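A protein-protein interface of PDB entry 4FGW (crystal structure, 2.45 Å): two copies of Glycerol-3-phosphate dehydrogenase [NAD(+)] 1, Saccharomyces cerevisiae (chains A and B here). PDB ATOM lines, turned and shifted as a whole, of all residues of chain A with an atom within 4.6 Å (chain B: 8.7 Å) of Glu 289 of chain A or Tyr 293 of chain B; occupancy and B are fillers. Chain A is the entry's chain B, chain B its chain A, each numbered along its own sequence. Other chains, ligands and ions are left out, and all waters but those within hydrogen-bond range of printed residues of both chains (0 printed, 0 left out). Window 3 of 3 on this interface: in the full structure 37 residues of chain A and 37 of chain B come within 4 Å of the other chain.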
ATOM      1  N   LEU A 273      10.577  27.580 -19.833  1.00  0.00           N
ATOM      2  CA  LEU A 273      11.189  27.235 -18.537  1.00  0.00           C
ATOM      3  C   LEU A 273      10.947  25.757 -18.197  1.00  0.00           C
ATOM      4  O   LEU A 273      11.882  25.072 -17.811  1.00  0.00           O
ATOM      5  CB  LEU A 273      10.692  28.147 -17.385  1.00  0.00           C
ATOM      6  CG  LEU A 273      11.386  27.956 -16.007  1.00  0.00           C
ATOM      7  CD1 LEU A 273      12.902  28.314 -16.065  1.00  0.00           C
ATOM      8  CD2 LEU A 273      10.679  28.732 -14.925  1.00  0.00           C
ATOM      9  N   ILE A 277      13.851  22.779 -17.762  1.00  0.00           N
ATOM     10  CA  ILE A 277      13.896  21.904 -16.576  1.00  0.00           C
ATOM     11  C   ILE A 277      13.879  20.432 -17.012  1.00  0.00           C
ATOM     12  O   ILE A 277      14.739  19.662 -16.588  1.00  0.00           O
ATOM     13  CB  ILE A 277      12.744  22.229 -15.577  1.00  0.00           C
ATOM     14  CG1 ILE A 277      12.912  23.648 -14.987  1.00  0.00           C
ATOM     15  CG2 ILE A 277      12.659  21.177 -14.464  1.00  0.00           C
ATOM     16  CD1 ILE A 277      11.640  24.307 -14.466  1.00  0.00           C
ATOM     17  N   GLN A 281      16.864  17.581 -16.465  1.00  0.00           N
ATOM     18  CA  GLN A 281      16.659  16.384 -15.664  1.00  0.00           C
ATOM     19  C   GLN A 281      16.740  15.093 -16.486  1.00  0.00           C
ATOM     20  O   GLN A 281      17.143  14.052 -15.956  1.00  0.00           O
ATOM     21  CB  GLN A 281      15.348  16.485 -14.888  1.00  0.00           C
ATOM     22  CG  GLN A 281      15.324  17.712 -13.980  1.00  0.00           C
ATOM     23  CD  GLN A 281      14.405  17.541 -12.821  1.00  0.00           C
ATOM     24  OE1 GLN A 281      13.174  17.579 -12.957  1.00  0.00           O
ATOM     25  NE2 GLN A 281      14.991  17.391 -11.643  1.00  0.00           N
ATOM     26  N   SER A 287      20.839  17.235 -12.020  1.00  0.00           N
ATOM     27  CA  SER A 287      20.545  18.639 -11.968  1.00  0.00           C
ATOM     28  C   SER A 287      19.387  18.876 -11.045  1.00  0.00           C
ATOM     29  O   SER A 287      18.468  18.103 -11.040  1.00  0.00           O
ATOM     30  CB  SER A 287      20.155  19.082 -13.362  1.00  0.00           C
ATOM     31  OG  SER A 287      20.351  20.440 -13.467  1.00  0.00           O
ATOM     32  N   ARG A 288      19.415  19.973 -10.308  1.00  0.00           N
ATOM     33  CA  ARG A 288      18.336  20.282  -9.381  1.00  0.00           C
ATOM     34  C   ARG A 288      17.337  21.202 -10.069  1.00  0.00           C
ATOM     35  O   ARG A 288      17.757  22.149 -10.741  1.00  0.00           O
ATOM     36  CB  ARG A 288      18.910  20.955  -8.126  1.00  0.00           C
ATOM     37  CG  ARG A 288      19.894  20.063  -7.358  1.00  0.00           C
ATOM     38  CD  ARG A 288      20.352  20.692  -6.061  1.00  0.00           C
ATOM     39  NE  ARG A 288      19.308  20.657  -5.031  1.00  0.00           N
ATOM     40  CZ  ARG A 288      18.811  21.733  -4.430  1.00  0.00           C
ATOM     41  NH1 ARG A 288      19.262  22.944  -4.741  1.00  0.00           N
ATOM     42  NH2 ARG A 288      17.866  21.607  -3.507  1.00  0.00           N
ATOM     43  N   GLU A 289      16.022  20.931  -9.911  1.00  0.00           N
ATOM     44  CA  GLU A 289      14.936  21.762 -10.459  1.00  0.00           C
ATOM     45  C   GLU A 289      15.081  23.194  -9.964  1.00  0.00           C
ATOM     46  O   GLU A 289      14.846  24.128 -10.725  1.00  0.00           O
ATOM     47  CB  GLU A 289      13.563  21.231 -10.013  1.00  0.00           C
ATOM     48  CG  GLU A 289      13.020  20.137 -10.906  1.00  0.00           C
ATOM     49  CD  GLU A 289      11.559  19.775 -10.735  1.00  0.00           C
ATOM     50  OE1 GLU A 289      10.688  20.654 -10.940  1.00  0.00           O
ATOM     51  OE2 GLU A 289      11.283  18.581 -10.476  1.00  0.00           O
ATOM     52  N   GLU A 290      15.490  23.344  -8.681  1.00  0.00           N
ATOM     53  CA  GLU A 290      15.716  24.578  -7.929  1.00  0.00           C
ATOM     54  C   GLU A 290      16.570  25.579  -8.680  1.00  0.00           C
ATOM     55  O   GLU A 290      16.222  26.749  -8.718  1.00  0.00           O
ATOM     56  CB  GLU A 290      16.342  24.262  -6.556  1.00  0.00           C
ATOM     57  CG  GLU A 290      15.355  23.698  -5.545  1.00  0.00           C
ATOM     58  CD  GLU A 290      15.047  22.212  -5.626  1.00  0.00           C
ATOM     59  OE1 GLU A 290      14.270  21.727  -4.769  1.00  0.00           O
ATOM     60  OE2 GLU A 290      15.578  21.530  -6.533  1.00  0.00           O
ATOM     61  N   THR A 291      17.659  25.109  -9.305  1.00  0.00           N
ATOM     62  CA  THR A 291      18.616  25.893 -10.086  1.00  0.00           C
ATOM     63  C   THR A 291      17.908  26.731 -11.161  1.00  0.00           C
ATOM     64  O   THR A 291      18.212  27.916 -11.317  1.00  0.00           O
ATOM     65  CB  THR A 291      19.656  24.937 -10.696  1.00  0.00           C
ATOM     66  OG1 THR A 291      20.236  24.162  -9.646  1.00  0.00           O
ATOM     67  CG2 THR A 291      20.742  25.656 -11.475  1.00  0.00           C
ATOM     68  N   TYR A 292      16.966  26.107 -11.880  1.00  0.00           N
ATOM     69  CA  TYR A 292      16.238  26.715 -12.993  1.00  0.00           C
ATOM     70  C   TYR A 292      15.317  27.874 -12.601  1.00  0.00           C
ATOM     71  O   TYR A 292      15.263  28.859 -13.326  1.00  0.00           O
ATOM     72  CB  TYR A 292      15.493  25.638 -13.793  1.00  0.00           C
ATOM     73  CG  TYR A 292      16.412  24.543 -14.295  1.00  0.00           C
ATOM     74  CD1 TYR A 292      17.089  24.676 -15.498  1.00  0.00           C
ATOM     75  CD2 TYR A 292      16.606  23.376 -13.562  1.00  0.00           C
ATOM     76  CE1 TYR A 292      17.956  23.690 -15.954  1.00  0.00           C
ATOM     77  CE2 TYR A 292      17.461  22.373 -14.014  1.00  0.00           C
ATOM     78  CZ  TYR A 292      18.133  22.537 -15.213  1.00  0.00           C
ATOM     79  OH  TYR A 292      18.989  21.577 -15.681  1.00  0.00           O
ATOM     80  N   TYR A 293      14.626  27.776 -11.452  1.00  0.00           N
ATOM     81  CA  TYR A 293      13.728  28.838 -11.004  1.00  0.00           C
ATOM     82  C   TYR A 293      14.269  29.736  -9.872  1.00  0.00           C
ATOM     83  O   TYR A 293      13.723  30.811  -9.661  1.00  0.00           O
ATOM     84  CB  TYR A 293      12.328  28.289 -10.694  1.00  0.00           C
ATOM     85  CG  TYR A 293      12.258  27.378  -9.489  1.00  0.00           C
ATOM     86  CD1 TYR A 293      12.427  26.002  -9.619  1.00  0.00           C
ATOM     87  CD2 TYR A 293      11.948  27.882  -8.224  1.00  0.00           C
ATOM     88  CE1 TYR A 293      12.325  25.154  -8.515  1.00  0.00           C
ATOM     89  CE2 TYR A 293      11.870  27.048  -7.115  1.00  0.00           C
ATOM     90  CZ  TYR A 293      12.051  25.684  -7.267  1.00  0.00           C
ATOM     91  OH  TYR A 293      11.966  24.848  -6.181  1.00  0.00           O
ATOM     92  N   GLY B 237      -1.607  28.783  -3.718  1.00  0.00           N
ATOM     93  CA  GLY B 237      -0.496  29.196  -4.581  1.00  0.00           C
ATOM     94  C   GLY B 237      -0.888  30.156  -5.686  1.00  0.00           C
ATOM     95  O   GLY B 237      -0.311  31.243  -5.791  1.00  0.00           O
ATOM     96  N   CYS B 241       0.077  34.814  -5.675  1.00  0.00           N
ATOM     97  CA  CYS B 241       0.797  35.349  -6.832  1.00  0.00           C
ATOM     98  C   CYS B 241       0.096  36.589  -7.392  1.00  0.00           C
ATOM     99  O   CYS B 241       0.764  37.584  -7.640  1.00  0.00           O
ATOM    100  CB  CYS B 241       0.944  34.278  -7.907  1.00  0.00           C
ATOM    101  SG  CYS B 241       2.001  32.884  -7.446  1.00  0.00           S
ATOM    102  N   LEU B 273      10.063  36.313  -7.252  1.00  0.00           N
ATOM    103  CA  LEU B 273       9.527  34.948  -7.356  1.00  0.00           C
ATOM    104  C   LEU B 273       9.877  34.133  -6.107  1.00  0.00           C
ATOM    105  O   LEU B 273       8.998  33.472  -5.559  1.00  0.00           O
ATOM    106  CB  LEU B 273       9.999  34.224  -8.641  1.00  0.00           C
ATOM    107  CG  LEU B 273       9.393  32.825  -8.912  1.00  0.00           C
ATOM    108  CD1 LEU B 273       7.870  32.886  -9.139  1.00  0.00           C
ATOM    109  CD2 LEU B 273      10.087  32.151 -10.066  1.00  0.00           C
ATOM    110  N   GLY B 274      11.127  34.235  -5.646  1.00  0.00           N
ATOM    111  CA  GLY B 274      11.600  33.553  -4.442  1.00  0.00           C
ATOM    112  C   GLY B 274      10.829  33.976  -3.207  1.00  0.00           C
ATOM    113  O   GLY B 274      10.483  33.135  -2.376  1.00  0.00           O
ATOM    114  N   ILE B 276       7.687  35.272  -3.202  1.00  0.00           N
ATOM    115  CA  ILE B 276       6.307  34.810  -3.401  1.00  0.00           C
ATOM    116  C   ILE B 276       6.215  33.339  -2.946  1.00  0.00           C
ATOM    117  O   ILE B 276       5.287  32.987  -2.224  1.00  0.00           O
ATOM    118  CB  ILE B 276       5.834  35.031  -4.872  1.00  0.00           C
ATOM    119  CG1 ILE B 276       5.780  36.551  -5.209  1.00  0.00           C
ATOM    120  CG2 ILE B 276       4.466  34.362  -5.121  1.00  0.00           C
ATOM    121  CD1 ILE B 276       5.533  36.933  -6.708  1.00  0.00           C
ATOM    122  N   ILE B 277       7.201  32.500  -3.331  1.00  0.00           N
ATOM    123  CA  ILE B 277       7.268  31.086  -2.926  1.00  0.00           C
ATOM    124  C   ILE B 277       7.361  30.986  -1.402  1.00  0.00           C
ATOM    125  O   ILE B 277       6.586  30.250  -0.783  1.00  0.00           O
ATOM    126  CB  ILE B 277       8.447  30.343  -3.634  1.00  0.00           C
ATOM    127  CG1 ILE B 277       8.220  30.271  -5.158  1.00  0.00           C
ATOM    128  CG2 ILE B 277       8.686  28.948  -3.029  1.00  0.00           C
ATOM    129  CD1 ILE B 277       9.466  30.104  -6.013  1.00  0.00           C
ATOM    130  N   GLN B 281       4.488  29.301   1.172  1.00  0.00           N
ATOM    131  CA  GLN B 281       4.817  28.144   2.004  1.00  0.00           C
ATOM    132  C   GLN B 281       4.889  28.428   3.497  1.00  0.00           C
ATOM    133  O   GLN B 281       4.718  27.506   4.301  1.00  0.00           O
ATOM    134  CB  GLN B 281       6.087  27.465   1.499  1.00  0.00           C
ATOM    135  CG  GLN B 281       5.951  26.982   0.061  1.00  0.00           C
ATOM    136  CD  GLN B 281       7.057  26.049  -0.300  1.00  0.00           C
ATOM    137  OE1 GLN B 281       8.243  26.405  -0.264  1.00  0.00           O
ATOM    138  NE2 GLN B 281       6.684  24.832  -0.660  1.00  0.00           N
ATOM    139  N   ARG B 288       2.257  24.202  -2.991  1.00  0.00           N
ATOM    140  CA  ARG B 288       3.359  23.519  -3.653  1.00  0.00           C
ATOM    141  C   ARG B 288       4.252  24.544  -4.324  1.00  0.00           C
ATOM    142  O   ARG B 288       3.738  25.464  -4.957  1.00  0.00           O
ATOM    143  CB  ARG B 288       2.808  22.522  -4.687  1.00  0.00           C
ATOM    144  CG  ARG B 288       1.934  21.430  -4.070  1.00  0.00           C
ATOM    145  CD  ARG B 288       1.493  20.393  -5.079  1.00  0.00           C
ATOM    146  NE  ARG B 288       2.584  19.489  -5.448  1.00  0.00           N
ATOM    147  CZ  ARG B 288       3.036  19.324  -6.687  1.00  0.00           C
ATOM    148  NH1 ARG B 288       2.487  19.990  -7.699  1.00  0.00           N
ATOM    149  NH2 ARG B 288       4.031  18.481  -6.929  1.00  0.00           N
ATOM    150  N   GLU B 289       5.589  24.391  -4.193  1.00  0.00           N
ATOM    151  CA  GLU B 289       6.586  25.262  -4.840  1.00  0.00           C
ATOM    152  C   GLU B 289       6.363  25.277  -6.347  1.00  0.00           C
ATOM    153  O   GLU B 289       6.491  26.325  -6.973  1.00  0.00           O
ATOM    154  CB  GLU B 289       8.011  24.755  -4.568  1.00  0.00           C
ATOM    155  CG  GLU B 289       8.605  25.245  -3.267  1.00  0.00           C
ATOM    156  CD  GLU B 289      10.099  25.048  -3.088  1.00  0.00           C
ATOM    157  OE1 GLU B 289      10.881  25.626  -3.881  1.00  0.00           O
ATOM    158  OE2 GLU B 289      10.488  24.376  -2.106  1.00  0.00           O
ATOM    159  N   GLU B 290       6.003  24.101  -6.906  1.00  0.00           N
ATOM    160  CA  GLU B 290       5.729  23.800  -8.308  1.00  0.00           C
ATOM    161  C   GLU B 290       4.772  24.781  -8.948  1.00  0.00           C
ATOM    162  O   GLU B 290       5.036  25.254 -10.046  1.00  0.00           O
ATOM    163  CB  GLU B 290       5.202  22.358  -8.453  1.00  0.00           C
ATOM    164  CG  GLU B 290       6.277  21.286  -8.324  1.00  0.00           C
ATOM    165  CD  GLU B 290       6.687  20.877  -6.917  1.00  0.00           C
ATOM    166  OE1 GLU B 290       7.531  19.959  -6.805  1.00  0.00           O
ATOM    167  OE2 GLU B 290       6.171  21.458  -5.933  1.00  0.00           O
ATOM    168  N   THR B 291       3.689  25.122  -8.241  1.00  0.00           N
ATOM    169  CA  THR B 291       2.643  26.056  -8.663  1.00  0.00           C
ATOM    170  C   THR B 291       3.224  27.398  -9.111  1.00  0.00           C
ATOM    171  O   THR B 291       2.833  27.922 -10.154  1.00  0.00           O
ATOM    172  CB  THR B 291       1.635  26.225  -7.497  1.00  0.00           C
ATOM    173  OG1 THR B 291       1.172  24.934  -7.100  1.00  0.00           O
ATOM    174  CG2 THR B 291       0.461  27.113  -7.848  1.00  0.00           C
ATOM    175  N   TYR B 292       4.163  27.934  -8.322  1.00  0.00           N
ATOM    176  CA  TYR B 292       4.792  29.232  -8.547  1.00  0.00           C
ATOM    177  C   TYR B 292       5.652  29.326  -9.812  1.00  0.00           C
ATOM    178  O   TYR B 292       5.609  30.352 -10.485  1.00  0.00           O
ATOM    179  CB  TYR B 292       5.566  29.668  -7.299  1.00  0.00           C
ATOM    180  CG  TYR B 292       4.705  29.701  -6.057  1.00  0.00           C
ATOM    181  CD1 TYR B 292       3.954  30.825  -5.738  1.00  0.00           C
ATOM    182  CD2 TYR B 292       4.629  28.603  -5.205  1.00  0.00           C
ATOM    183  CE1 TYR B 292       3.132  30.852  -4.615  1.00  0.00           C
ATOM    184  CE2 TYR B 292       3.818  28.621  -4.071  1.00  0.00           C
ATOM    185  CZ  TYR B 292       3.072  29.750  -3.781  1.00  0.00           C
ATOM    186  OH  TYR B 292       2.267  29.786  -2.672  1.00  0.00           O
ATOM    187  N   TYR B 293       6.408  28.269 -10.145  1.00  0.00           N
ATOM    188  CA  TYR B 293       7.260  28.280 -11.336  1.00  0.00           C
ATOM    189  C   TYR B 293       6.726  27.497 -12.539  1.00  0.00           C
ATOM    190  O   TYR B 293       7.210  27.714 -13.643  1.00  0.00           O
ATOM    191  CB  TYR B 293       8.714  27.901 -10.995  1.00  0.00           C
ATOM    192  CG  TYR B 293       8.912  26.463 -10.564  1.00  0.00           C
ATOM    193  CD1 TYR B 293       8.828  26.099  -9.225  1.00  0.00           C
ATOM    194  CD2 TYR B 293       9.242  25.474 -11.490  1.00  0.00           C
ATOM    195  CE1 TYR B 293       9.037  24.783  -8.820  1.00  0.00           C
ATOM    196  CE2 TYR B 293       9.437  24.150 -11.097  1.00  0.00           C
ATOM    197  CZ  TYR B 293       9.342  23.811  -9.759  1.00  0.00           C
ATOM    198  OH  TYR B 293       9.542  22.512  -9.365  1.00  0.00           O
ATOM    199  N   GLN B 294       5.739  26.598 -12.341  1.00  0.00           N
ATOM    200  CA  GLN B 294       5.159  25.788 -13.426  1.00  0.00           C
ATOM    201  C   GLN B 294       3.891  26.371 -14.025  1.00  0.00           C
ATOM    202  O   GLN B 294       3.558  26.028 -15.158  1.00  0.00           O
ATOM    203  CB  GLN B 294       4.825  24.368 -12.944  1.00  0.00           C
ATOM    204  CG  GLN B 294       6.019  23.517 -12.534  1.00  0.00           C
ATOM    205  CD  GLN B 294       5.660  22.089 -12.188  1.00  0.00           C
ATOM    206  OE1 GLN B 294       6.520  21.210 -12.173  1.00  0.00           O
ATOM    207  NE2 GLN B 294       4.396  21.810 -11.887  1.00  0.00           N
ATOM    208  N   GLU B 295       3.144  27.195 -13.254  1.00  0.00           N
ATOM    209  CA  GLU B 295       1.836  27.690 -13.686  1.00  0.00           C
ATOM    210  C   GLU B 295       1.760  29.138 -14.147  1.00  0.00           C
ATOM    211  O   GLU B 295       2.579  29.976 -13.741  1.00  0.00           O
ATOM    212  CB  GLU B 295       0.747  27.374 -12.624  1.00  0.00           C
ATOM    213  CG  GLU B 295       0.709  25.920 -12.148  1.00  0.00           C
ATOM    214  CD  GLU B 295       0.464  24.843 -13.187  1.00  0.00           C
ATOM    215  OE1 GLU B 295      -0.179  25.139 -14.218  1.00  0.00           O
ATOM    216  OE2 GLU B 295       0.888  23.689 -12.958  1.00  0.00           O
ATOM    217  N   SER B 296       0.746  29.422 -15.001  1.00  0.00           N
ATOM    218  CA  SER B 296       0.452  30.746 -15.543  1.00  0.00           C
ATOM    219  C   SER B 296       0.240  31.759 -14.420  1.00  0.00           C
ATOM    220  O   SER B 296       0.744  32.877 -14.490  1.00  0.00           O
ATOM    221  CB  SER B 296      -0.774  30.693 -16.452  1.00  0.00           C
ATOM    222  OG  SER B 296      -1.004  31.952 -17.066  1.00  0.00           O
ATOM    223  N   ALA B 297      -0.479  31.338 -13.369  1.00  0.00           N
ATOM    224  CA  ALA B 297      -0.785  32.131 -12.183  1.00  0.00           C
ATOM    225  C   ALA B 297       0.485  32.599 -11.465  1.00  0.00           C
ATOM    226  O   ALA B 297       0.487  33.691 -10.905  1.00  0.00           O
ATOM    227  CB  ALA B 297      -1.635  31.314 -11.241  1.00  0.00           C
ATOM    228  N   GLY B 298       1.541  31.782 -11.526  1.00  0.00           N
ATOM    229  CA  GLY B 298       2.830  32.062 -10.914  1.00  0.00           C
ATOM    230  C   GLY B 298       3.738  32.903 -11.780  1.00  0.00           C
ATOM    231  O   GLY B 298       3.441  34.072 -12.033  1.00  0.00           O
ATOM    232  N   VAL B 299       4.846  32.290 -12.242  1.00  0.00           N
ATOM    233  CA  VAL B 299       5.906  32.890 -13.058  1.00  0.00           C
ATOM    234  C   VAL B 299       5.420  33.743 -14.259  1.00  0.00           C
ATOM    235  O   VAL B 299       5.891  34.876 -14.428  1.00  0.00           O
ATOM    236  CB  VAL B 299       7.003  31.842 -13.430  1.00  0.00           C
ATOM    237  CG1 VAL B 299       6.506  30.818 -14.458  1.00  0.00           C
ATOM    238  CG2 VAL B 299       8.283  32.520 -13.916  1.00  0.00           C
ATOM    239  N   ALA B 300       4.477  33.214 -15.069  1.00  0.00           N
ATOM    240  CA  ALA B 300       3.964  33.918 -16.255  1.00  0.00           C
ATOM    241  C   ALA B 300       3.248  35.223 -15.870  1.00  0.00           C
ATOM    242  O   ALA B 300       3.503  36.269 -16.482  1.00  0.00           O
ATOM    243  CB  ALA B 300       3.039  33.013 -17.061  1.00  0.00           C
ATOM    244  N   LEU B 302       3.764  36.965 -13.151  1.00  0.00           N
ATOM    245  CA  LEU B 302       4.830  37.835 -12.662  1.00  0.00           C
ATOM    246  C   LEU B 302       5.546  38.518 -13.853  1.00  0.00           C
ATOM    247  O   LEU B 302       5.718  39.734 -13.847  1.00  0.00           O
ATOM    248  CB  LEU B 302       5.825  37.016 -11.819  1.00  0.00           C
ATOM    249  CG  LEU B 302       6.996  37.786 -11.192  1.00  0.00           C
ATOM    250  CD1 LEU B 302       6.506  38.750 -10.104  1.00  0.00           C
ATOM    251  CD2 LEU B 302       8.036  36.838 -10.637  1.00  0.00           C
ATOM    252  N   ILE B 303       5.943  37.723 -14.872  1.00  0.00           N
ATOM    253  CA  ILE B 303       6.627  38.212 -16.069  1.00  0.00           C
ATOM    254  C   ILE B 303       5.819  39.305 -16.780  1.00  0.00           C
ATOM    255  O   ILE B 303       6.344  40.394 -16.994  1.00  0.00           O
ATOM    256  CB  ILE B 303       7.071  37.048 -17.017  1.00  0.00           C
ATOM    257  CG1 ILE B 303       8.186  36.207 -16.354  1.00  0.00           C
ATOM    258  CG2 ILE B 303       7.539  37.591 -18.397  1.00  0.00           C
ATOM    259  CD1 ILE B 303       8.493  34.829 -17.040  1.00  0.00           C
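OH of Tyr 293 of chain A lies within hydrogen-bond range of OE1 of Glu 289 of chain B (2.7 Å). The side-chain hydroxyl of Tyr 293 of chain B lies within hydrogen-bond range of the side-chain carboxylate of Glu 289 of chain A.
The side-chain carboxylate of Glu 289 of chain A lies close to the side-chain amide oxygen of Gln 281 of chain A.
Among the printed residues, pairs that only touch across the chains: Leu 273 of chain A with Tyr 293 of chain B (3.8 Å), Ile 277 of chain A with Tyr 293 of chain B (3.996 Å), Tyr 293 of chain A with Leu 273 of chain B (3.9 Å), Tyr 293 of chain A with Ile 277 of chain B (3.998 Å) and Tyr 293 of chain A with Tyr 293 of chain B (3.3 Å).
Of the printed residues of chain B, Glu 289 of chain A touches Tyr 293. Of the printed residues of chain A, Tyr 293 of chain B touches Leu 273, Ile 277, Glu 289 and Tyr 293. Of the printed residues of chain A, Leu 273 of chain B touches Tyr 293 (3.9 Å). Printed residues of chain B within 4 Å of Ile 277 of chain A: Tyr 293 (3.996 Å). Printed residues of chain B within 4 Å of Tyr 293 of chain A: Leu 273, Ile 277, Glu 289 and Tyr 293. Tyr 292 of chain B touches none of the printed residues of chain A. The nearest residue of chain B that does not touch Glu 289 of chain A is Gln 294 of chain B (4.4 Å). The nearest printed residue of chain A that does not touch Tyr 293 of chain B is Glu 290 of chain A (6.0 Å).
Of the 22 printed residues of chain B, 4 touch a printed residue of chain A. Hydrophobic or aromatic side chains of chain B that line the printed part of chain A: Leu 273, Ile 277 and Tyr 293. Hydrophobic or aromatic side chains of chain A within 4 Å of the printed part of chain B: Leu 273, Ile 277 and Tyr 293. Among the printed residues, no Asp or Glu carboxylate lies within 4 Å of a Lys or Arg side-chain nitrogen of the other chain.
Leu 273 of chain A touches Tyr 293 of chain B, and with the chains exchanged Tyr 293 of chain A touches Leu 273 of chain B. Ile 277 of chain A touches Tyr 293 of chain B, and with the chains exchanged Tyr 293 of chain A touches Ile 277 of chain B. Glu 289 of chain A touches Tyr 293 of chain B, and with the chains exchanged Tyr 293 of chain A touches Glu 289 of chain B. Tyr 293 of chain A touches its own counterpart, Tyr 293 of chain B.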
